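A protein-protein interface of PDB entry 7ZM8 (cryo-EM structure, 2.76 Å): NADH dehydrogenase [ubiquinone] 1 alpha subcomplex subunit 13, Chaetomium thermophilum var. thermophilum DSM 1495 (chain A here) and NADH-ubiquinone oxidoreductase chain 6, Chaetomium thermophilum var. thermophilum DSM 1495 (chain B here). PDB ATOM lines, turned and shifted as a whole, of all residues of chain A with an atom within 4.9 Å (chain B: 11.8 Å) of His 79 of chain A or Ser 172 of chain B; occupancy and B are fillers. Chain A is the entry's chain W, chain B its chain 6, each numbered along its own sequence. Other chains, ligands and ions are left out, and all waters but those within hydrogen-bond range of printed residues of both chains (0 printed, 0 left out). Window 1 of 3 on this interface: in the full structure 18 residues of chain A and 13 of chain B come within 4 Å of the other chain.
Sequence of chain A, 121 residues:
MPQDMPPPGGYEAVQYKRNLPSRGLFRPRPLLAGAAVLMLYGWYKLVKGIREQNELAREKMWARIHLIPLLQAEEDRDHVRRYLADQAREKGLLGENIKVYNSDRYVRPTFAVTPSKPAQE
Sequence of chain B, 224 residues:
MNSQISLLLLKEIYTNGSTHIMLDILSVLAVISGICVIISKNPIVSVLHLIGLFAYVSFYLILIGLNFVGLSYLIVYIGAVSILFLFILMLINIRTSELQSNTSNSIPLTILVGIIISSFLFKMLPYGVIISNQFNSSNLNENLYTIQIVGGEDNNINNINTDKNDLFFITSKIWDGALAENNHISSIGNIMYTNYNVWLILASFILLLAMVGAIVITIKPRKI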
ATOM      1  N   GLU A  75      24.674  -4.910  27.828  1.00  0.00           N
ATOM      2  CA  GLU A  75      25.058  -3.508  27.731  1.00  0.00           C
ATOM      3  C   GLU A  75      25.906  -3.249  26.490  1.00  0.00           C
ATOM      4  O   GLU A  75      25.762  -2.207  25.841  1.00  0.00           O
ATOM      5  CB  GLU A  75      25.805  -3.093  28.994  1.00  0.00           C
ATOM      6  CG  GLU A  75      25.916  -1.584  29.219  1.00  0.00           C
ATOM      7  CD  GLU A  75      24.598  -0.929  29.604  1.00  0.00           C
ATOM      8  OE1 GLU A  75      23.701  -1.628  30.128  1.00  0.00           O
ATOM      9  OE2 GLU A  75      24.463   0.295  29.391  1.00  0.00           O
ATOM     10  N   ASP A  76      26.788  -4.189  26.142  1.00  0.00           N
ATOM     11  CA  ASP A  76      27.707  -3.986  25.026  1.00  0.00           C
ATOM     12  C   ASP A  76      26.981  -3.969  23.689  1.00  0.00           C
ATOM     13  O   ASP A  76      27.368  -3.227  22.781  1.00  0.00           O
ATOM     14  CB  ASP A  76      28.781  -5.066  25.027  1.00  0.00           C
ATOM     15  CG  ASP A  76      29.812  -4.844  26.093  1.00  0.00           C
ATOM     16  OD1 ASP A  76      29.794  -3.758  26.703  1.00  0.00           O
ATOM     17  OD2 ASP A  76      30.641  -5.747  26.324  1.00  0.00           O
ATOM     18  N   ARG A  77      25.950  -4.796  23.535  1.00  0.00           N
ATOM     19  CA  ARG A  77      25.170  -4.749  22.306  1.00  0.00           C
ATOM     20  C   ARG A  77      24.410  -3.438  22.199  1.00  0.00           C
ATOM     21  O   ARG A  77      24.225  -2.908  21.100  1.00  0.00           O
ATOM     22  CB  ARG A  77      24.215  -5.934  22.243  1.00  0.00           C
ATOM     23  CG  ARG A  77      24.911  -7.258  22.125  1.00  0.00           C
ATOM     24  CD  ARG A  77      23.934  -8.401  22.082  1.00  0.00           C
ATOM     25  NE  ARG A  77      23.367  -8.705  23.389  1.00  0.00           N
ATOM     26  CZ  ARG A  77      23.763  -9.710  24.161  1.00  0.00           C
ATOM     27  NH1 ARG A  77      24.738 -10.514  23.772  1.00  0.00           N
ATOM     28  NH2 ARG A  77      23.180  -9.908  25.331  1.00  0.00           N
ATOM     29  N   ASP A  78      23.967  -2.902  23.335  1.00  0.00           N
ATOM     30  CA  ASP A  78      23.269  -1.626  23.333  1.00  0.00           C
ATOM     31  C   ASP A  78      24.206  -0.488  22.953  1.00  0.00           C
ATOM     32  O   ASP A  78      23.813   0.431  22.231  1.00  0.00           O
ATOM     33  CB  ASP A  78      22.651  -1.379  24.705  1.00  0.00           C
ATOM     34  CG  ASP A  78      21.467  -0.452  24.652  1.00  0.00           C
ATOM     35  OD1 ASP A  78      20.464  -0.815  24.008  1.00  0.00           O
ATOM     36  OD2 ASP A  78      21.531   0.634  25.262  1.00  0.00           O
ATOM     37  N   HIS A  79      25.449  -0.537  23.409  1.00  0.00           N
ATOM     38  CA  HIS A  79      26.452   0.490  23.049  1.00  0.00           C
ATOM     39  C   HIS A  79      26.822   0.344  21.581  1.00  0.00           C
ATOM     40  O   HIS A  79      27.010   1.370  20.928  1.00  0.00           O
ATOM     41  CB  HIS A  79      27.664   0.408  23.972  1.00  0.00           C
ATOM     42  CG  HIS A  79      27.407   0.979  25.319  1.00  0.00           C
ATOM     43  ND1 HIS A  79      28.006   2.132  25.751  1.00  0.00           N
ATOM     44  CD2 HIS A  79      26.595   0.575  26.316  1.00  0.00           C
ATOM     45  CE1 HIS A  79      27.595   2.398  26.964  1.00  0.00           C
ATOM     46  NE2 HIS A  79      26.726   1.469  27.332  1.00  0.00           N
ATOM     47  N   VAL A  80      26.937  -0.886  21.086  1.00  0.00           N
ATOM     48  CA  VAL A  80      27.200  -1.079  19.632  1.00  0.00           C
ATOM     49  C   VAL A  80      25.992  -0.533  18.860  1.00  0.00           C
ATOM     50  O   VAL A  80      26.215   0.215  17.903  1.00  0.00           O
ATOM     51  CB  VAL A  80      27.522  -2.552  19.302  1.00  0.00           C
ATOM     52  CG1 VAL A  80      27.522  -2.825  17.809  1.00  0.00           C
ATOM     53  CG2 VAL A  80      28.840  -2.989  19.918  1.00  0.00           C
ATOM     54  N   ARG A  81      24.770  -0.874  19.280  1.00  0.00           N
ATOM     55  CA  ARG A  81      23.551  -0.415  18.566  1.00  0.00           C
ATOM     56  C   ARG A  81      23.500   1.103  18.423  1.00  0.00           C
ATOM     57  O   ARG A  81      23.352   1.589  17.299  1.00  0.00           O
ATOM     58  CB  ARG A  81      22.294  -0.944  19.250  1.00  0.00           C
ATOM     59  CG  ARG A  81      21.057  -1.031  18.376  1.00  0.00           C
ATOM     60  CD  ARG A  81      19.946  -1.646  19.199  1.00  0.00           C
ATOM     61  NE  ARG A  81      19.819  -0.972  20.479  1.00  0.00           N
ATOM     62  CZ  ARG A  81      19.220   0.197  20.650  1.00  0.00           C
ATOM     63  NH1 ARG A  81      19.147   0.743  21.850  1.00  0.00           N
ATOM     64  NH2 ARG A  81      18.703   0.823  19.610  1.00  0.00           N
ATOM     65  N   ARG A  82      23.602   1.838  19.523  1.00  0.00           N
ATOM     66  CA  ARG A  82      23.406   3.305  19.440  1.00  0.00           C
ATOM     67  C   ARG A  82      24.525   3.968  18.662  1.00  0.00           C
ATOM     68  O   ARG A  82      24.264   4.990  18.039  1.00  0.00           O
ATOM     69  CB  ARG A  82      23.217   3.826  20.868  1.00  0.00           C
ATOM     70  CG  ARG A  82      22.048   3.154  21.573  1.00  0.00           C
ATOM     71  CD  ARG A  82      21.526   3.818  22.826  1.00  0.00           C
ATOM     72  NE  ARG A  82      21.190   5.216  22.633  1.00  0.00           N
ATOM     73  CZ  ARG A  82      20.325   5.880  23.380  1.00  0.00           C
ATOM     74  NH1 ARG A  82      20.080   7.154  23.136  1.00  0.00           N
ATOM     75  NH2 ARG A  82      19.690   5.265  24.355  1.00  0.00           N
ATOM     76  N   TYR A  83      25.736   3.442  18.788  1.00  0.00           N
ATOM     77  CA  TYR A  83      26.904   4.027  18.099  1.00  0.00           C
ATOM     78  C   TYR A  83      26.740   3.874  16.595  1.00  0.00           C
ATOM     79  O   TYR A  83      27.010   4.813  15.869  1.00  0.00           O
ATOM     80  CB  TYR A  83      28.194   3.403  18.623  1.00  0.00           C
ATOM     81  CG  TYR A  83      29.421   3.748  17.817  1.00  0.00           C
ATOM     82  CD1 TYR A  83      30.143   4.898  18.075  1.00  0.00           C
ATOM     83  CD2 TYR A  83      29.842   2.939  16.777  1.00  0.00           C
ATOM     84  CE1 TYR A  83      31.257   5.232  17.325  1.00  0.00           C
ATOM     85  CE2 TYR A  83      30.951   3.258  16.017  1.00  0.00           C
ATOM     86  CZ  TYR A  83      31.661   4.408  16.294  1.00  0.00           C
ATOM     87  OH  TYR A  83      32.758   4.722  15.548  1.00  0.00           O
ATOM     88  N   TYR A 106      36.698   2.771  21.204  1.00  0.00           N
ATOM     89  CA  TYR A 106      35.299   3.200  21.437  1.00  0.00           C
ATOM     90  C   TYR A 106      35.290   4.028  22.707  1.00  0.00           C
ATOM     91  O   TYR A 106      35.632   3.523  23.776  1.00  0.00           O
ATOM     92  CB  TYR A 106      34.317   2.035  21.573  1.00  0.00           C
ATOM     93  CG  TYR A 106      32.973   2.445  22.115  1.00  0.00           C
ATOM     94  CD1 TYR A 106      32.150   3.302  21.407  1.00  0.00           C
ATOM     95  CD2 TYR A 106      32.537   1.997  23.350  1.00  0.00           C
ATOM     96  CE1 TYR A 106      30.925   3.701  21.906  1.00  0.00           C
ATOM     97  CE2 TYR A 106      31.315   2.387  23.864  1.00  0.00           C
ATOM     98  CZ  TYR A 106      30.506   3.238  23.138  1.00  0.00           C
ATOM     99  OH  TYR A 106      29.301   3.621  23.644  1.00  0.00           O
ATOM    100  N   ARG A 108      32.815   6.050  25.242  1.00  0.00           N
ATOM    101  CA  ARG A 108      31.371   6.104  25.593  1.00  0.00           C
ATOM    102  C   ARG A 108      30.879   7.544  25.473  1.00  0.00           C
ATOM    103  O   ARG A 108      31.535   8.409  26.074  1.00  0.00           O
ATOM    104  CB  ARG A 108      31.101   5.461  26.957  1.00  0.00           C
ATOM    105  CG  ARG A 108      31.375   3.968  27.024  1.00  0.00           C
ATOM    106  CD  ARG A 108      31.567   3.524  28.458  1.00  0.00           C
ATOM    107  NE  ARG A 108      30.331   3.524  29.219  1.00  0.00           N
ATOM    108  CZ  ARG A 108      29.598   2.445  29.462  1.00  0.00           C
ATOM    109  NH1 ARG A 108      28.482   2.550  30.163  1.00  0.00           N
ATOM    110  NH2 ARG A 108      29.980   1.270  28.998  1.00  0.00           N
ATOM    111  N   LEU B   7      15.068   8.717  17.796  1.00  0.00           N
ATOM    112  CA  LEU B   7      15.452   9.273  19.113  1.00  0.00           C
ATOM    113  C   LEU B   7      14.182   9.738  19.817  1.00  0.00           C
ATOM    114  O   LEU B   7      13.435  10.504  19.211  1.00  0.00           O
ATOM    115  CB  LEU B   7      16.444  10.425  18.930  1.00  0.00           C
ATOM    116  CG  LEU B   7      17.777  10.080  18.278  1.00  0.00           C
ATOM    117  CD1 LEU B   7      18.571  11.350  18.024  1.00  0.00           C
ATOM    118  CD2 LEU B   7      18.572   9.116  19.144  1.00  0.00           C
ATOM    119  N   GLU B  12      11.888  11.150  33.315  1.00  0.00           N
ATOM    120  CA  GLU B  12      12.053  10.059  34.312  1.00  0.00           C
ATOM    121  C   GLU B  12      11.028  10.218  35.437  1.00  0.00           C
ATOM    122  O   GLU B  12      10.651  11.365  35.726  1.00  0.00           O
ATOM    123  CB  GLU B  12      13.476  10.066  34.856  1.00  0.00           C
ATOM    124  CG  GLU B  12      14.518  10.277  33.782  1.00  0.00           C
ATOM    125  CD  GLU B  12      15.930  10.370  34.321  1.00  0.00           C
ATOM    126  OE1 GLU B  12      16.839  10.713  33.548  1.00  0.00           O
ATOM    127  OE2 GLU B  12      16.112  10.093  35.513  1.00  0.00           O
ATOM    128  N   PHE B 168      23.345  18.254  25.745  1.00  0.00           N
ATOM    129  CA  PHE B 168      22.868  17.562  26.962  1.00  0.00           C
ATOM    130  C   PHE B 168      23.945  16.535  27.296  1.00  0.00           C
ATOM    131  O   PHE B 168      24.563  16.026  26.366  1.00  0.00           O
ATOM    132  CB  PHE B 168      21.510  16.903  26.717  1.00  0.00           C
ATOM    133  CG  PHE B 168      20.309  17.793  26.912  1.00  0.00           C
ATOM    134  CD1 PHE B 168      19.872  18.632  25.902  1.00  0.00           C
ATOM    135  CD2 PHE B 168      19.603  17.775  28.103  1.00  0.00           C
ATOM    136  CE1 PHE B 168      18.764  19.444  26.082  1.00  0.00           C
ATOM    137  CE2 PHE B 168      18.494  18.587  28.283  1.00  0.00           C
ATOM    138  CZ  PHE B 168      18.077  19.420  27.272  1.00  0.00           C
ATOM    139  N   PHE B 169      24.129  16.225  28.578  1.00  0.00           N
ATOM    140  CA  PHE B 169      25.151  15.238  29.007  1.00  0.00           C
ATOM    141  C   PHE B 169      24.484  13.871  29.125  1.00  0.00           C
ATOM    142  O   PHE B 169      23.598  13.712  29.965  1.00  0.00           O
ATOM    143  CB  PHE B 169      25.749  15.647  30.353  1.00  0.00           C
ATOM    144  CG  PHE B 169      26.780  16.739  30.286  1.00  0.00           C
ATOM    145  CD1 PHE B 169      28.113  16.437  30.063  1.00  0.00           C
ATOM    146  CD2 PHE B 169      26.419  18.064  30.454  1.00  0.00           C
ATOM    147  CE1 PHE B 169      29.064  17.442  30.006  1.00  0.00           C
ATOM    148  CE2 PHE B 169      27.370  19.067  30.396  1.00  0.00           C
ATOM    149  CZ  PHE B 169      28.690  18.753  30.173  1.00  0.00           C
ATOM    150  N   ILE B 170      24.907  12.921  28.298  1.00  0.00           N
ATOM    151  CA  ILE B 170      24.305  11.555  28.304  1.00  0.00           C
ATOM    152  C   ILE B 170      25.073  10.645  29.266  1.00  0.00           C
ATOM    153  O   ILE B 170      26.297  10.780  29.354  1.00  0.00           O
ATOM    154  CB  ILE B 170      24.185  10.971  26.878  1.00  0.00           C
ATOM    155  CG1 ILE B 170      23.242   9.768  26.818  1.00  0.00           C
ATOM    156  CG2 ILE B 170      25.541  10.666  26.266  1.00  0.00           C
ATOM    157  CD1 ILE B 170      21.792  10.141  26.660  1.00  0.00           C
ATOM    158  N   THR B 171      24.358   9.797  30.003  1.00  0.00           N
ATOM    159  CA  THR B 171      25.023   8.808  30.883  1.00  0.00           C
ATOM    160  C   THR B 171      24.351   7.446  30.735  1.00  0.00           C
ATOM    161  O   THR B 171      23.140   7.417  30.516  1.00  0.00           O
ATOM    162  CB  THR B 171      24.994   9.226  32.361  1.00  0.00           C
ATOM    163  OG1 THR B 171      23.685   9.677  32.705  1.00  0.00           O
ATOM    164  CG2 THR B 171      26.017  10.283  32.713  1.00  0.00           C
ATOM    165  N   SER B 172      25.113   6.363  30.859  1.00  0.00           N
ATOM    166  CA  SER B 172      24.558   5.017  30.830  1.00  0.00           C
ATOM    167  C   SER B 172      25.115   4.219  31.999  1.00  0.00           C
ATOM    168  O   SER B 172      25.858   4.760  32.822  1.00  0.00           O
ATOM    169  CB  SER B 172      24.877   4.329  29.505  1.00  0.00           C
ATOM    170  OG  SER B 172      24.771   2.925  29.623  1.00  0.00           O
ATOM    171  N   LYS B 173      24.748   2.935  32.098  1.00  0.00           N
ATOM    172  CA  LYS B 173      25.131   2.072  33.246  1.00  0.00           C
ATOM    173  C   LYS B 173      26.295   1.136  32.898  1.00  0.00           C
ATOM    174  O   LYS B 173      26.445   0.823  31.716  1.00  0.00           O
ATOM    175  CB  LYS B 173      23.874   1.296  33.649  1.00  0.00           C
ATOM    176  CG  LYS B 173      23.484   0.109  32.787  1.00  0.00           C
ATOM    177  CD  LYS B 173      22.368  -0.706  33.402  1.00  0.00           C
ATOM    178  CE  LYS B 173      21.287   0.144  34.037  1.00  0.00           C
ATOM    179  NZ  LYS B 173      20.052  -0.627  34.315  1.00  0.00           N
ATOM    180  N   ILE B 174      27.089   0.708  33.883  1.00  0.00           N
ATOM    181  CA  ILE B 174      28.199  -0.278  33.674  1.00  0.00           C
ATOM    182  C   ILE B 174      28.070  -1.355  34.748  1.00  0.00           C
ATOM    183  O   ILE B 174      27.521  -1.053  35.799  1.00  0.00           O
ATOM    184  CB  ILE B 174      29.599   0.380  33.716  1.00  0.00           C
ATOM    185  CG1 ILE B 174      30.702  -0.548  33.210  1.00  0.00           C
ATOM    186  CG2 ILE B 174      29.922   0.928  35.096  1.00  0.00           C
ATOM    187  CD1 ILE B 174      32.049   0.121  33.147  1.00  0.00           C
ATOM    188  N   TRP B 175      28.598  -2.553  34.509  1.00  0.00           N
ATOM    189  CA  TRP B 175      28.407  -3.660  35.480  1.00  0.00           C
ATOM    190  C   TRP B 175      29.734  -4.082  36.107  1.00  0.00           C
ATOM    191  O   TRP B 175      29.775  -4.259  37.333  1.00  0.00           O
ATOM    192  CB  TRP B 175      27.673  -4.822  34.811  1.00  0.00           C
ATOM    193  CG  TRP B 175      26.259  -4.466  34.477  1.00  0.00           C
ATOM    194  CD1 TRP B 175      25.763  -4.113  33.257  1.00  0.00           C
ATOM    195  CD2 TRP B 175      25.157  -4.382  35.397  1.00  0.00           C
ATOM    196  NE1 TRP B 175      24.426  -3.842  33.349  1.00  0.00           N
ATOM    197  CE2 TRP B 175      24.026  -3.995  34.650  1.00  0.00           C
ATOM    198  CE3 TRP B 175      25.014  -4.605  36.771  1.00  0.00           C
ATOM    199  CZ2 TRP B 175      22.771  -3.832  35.231  1.00  0.00           C
ATOM    200  CZ3 TRP B 175      23.775  -4.443  37.344  1.00  0.00           C
ATOM    201  CH2 TRP B 175      22.671  -4.066  36.582  1.00  0.00           C
ATOM    202  N   ASP B 176      30.771  -4.248  35.293  1.00  0.00           N
ATOM    203  CA  ASP B 176      32.110  -4.638  35.806  1.00  0.00           C
ATOM    204  C   ASP B 176      32.664  -3.538  36.724  1.00  0.00           C
ATOM    205  O   ASP B 176      33.320  -3.891  37.719  1.00  0.00           O
ATOM    206  CB  ASP B 176      33.033  -5.158  34.695  1.00  0.00           C
ATOM    207  CG  ASP B 176      33.026  -4.357  33.405  1.00  0.00           C
ATOM    208  OD1 ASP B 176      32.532  -3.217  33.420  1.00  0.00           O
ATOM    209  OD2 ASP B 176      33.525  -4.884  32.394  1.00  0.00           O
ATOM    210  N   GLY B 177      32.425  -2.269  36.395  1.00  0.00           N
ATOM    211  CA  GLY B 177      32.896  -1.144  37.224  1.00  0.00           C
ATOM    212  C   GLY B 177      31.948  -0.796  38.360  1.00  0.00           C
ATOM    213  O   GLY B 177      32.219   0.197  39.052  1.00  0.00           O
ATOM    214  N   ALA B 178      30.872  -1.561  38.546  1.00  0.00           N
ATOM    215  CA  ALA B 178      29.934  -1.355  39.672  1.00  0.00           C
ATOM    216  C   ALA B 178      30.006  -2.494  40.682  1.00  0.00           C
ATOM    217  O   ALA B 178      29.173  -2.463  41.590  1.00  0.00           O
ATOM    218  CB  ALA B 178      28.536  -1.252  39.123  1.00  0.00           C
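His 79 of chain A touches one residue of chain B. Of chain A, only Glu 75 (2.7 Å), His 79 (3.3 Å) and Arg 108 (3.8 Å) come within 4 Å of Ser 172 of chain B. Of chain B, only Ser 172 (2.7 Å), Lys 173 (3.1 Å) and Trp 175 (3.98 Å) come within 4 Å of Glu 75 of chain A. No residue of chain B comes within 4 Å of Asp 76 of chain A. No residue of chain B comes within 4 Å of Asp 78 of chain A. Printed residues of chain A within 4 Å of Lys 173 of chain B: Glu 75 (3.1 Å) and Arg 108 (3.1 Å). Of the printed residues of chain A, Trp 175 of chain B touches Glu 75. Arg 81 of chain A touches none of the printed residues of chain B.
Glu 75 of chain A touches Trp 175 of chain B. Ser 172 of chain B touches Arg 108 of chain A (OG to NH1, 3.8 Å).
The side-chain carboxylate of Glu 75 of chain A is in hydrogen-bond range of a ring nitrogen (NE2) of His 79 of chain A. ND1 of His 79 of chain A is in hydrogen-bond range of OH of Tyr 106 of chain A.
The backbone carbonyl oxygen (O) of Lys 173 of chain B lies close to the side-chain carboxylate (OE2) of Glu 75 of chain A (3.1 Å). The guanidinium group (NH1) of Arg 108 of chain A lies within hydrogen-bond range of the backbone carbonyl oxygen (O) of Lys 173 of chain B (3.1 Å). NE2 of His 79 of chain A sits at hydrogen-bond distance from OG of Ser 172 of chain B (3.3 Å). OE2 of Glu 75 of chain A sits at hydrogen-bond distance from OG of Ser 172 of chain B, 2.7 Å away.
Of the 11 printed residues of chain A, 3 touch a printed residue of chain B. Hydrophobic or aromatic side chains of chain A that line the printed part of chain B: His 79. Printed residues of chain B that touch a printed residue of chain A: Ser 172, Lys 173 and Trp 175. Among the printed residues, 6 pairs touch across the chains. Among the printed residues, no Asp or Glu carboxylate lies within 4 Å of a Lys or Arg side-chain nitrogen of the other chain.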
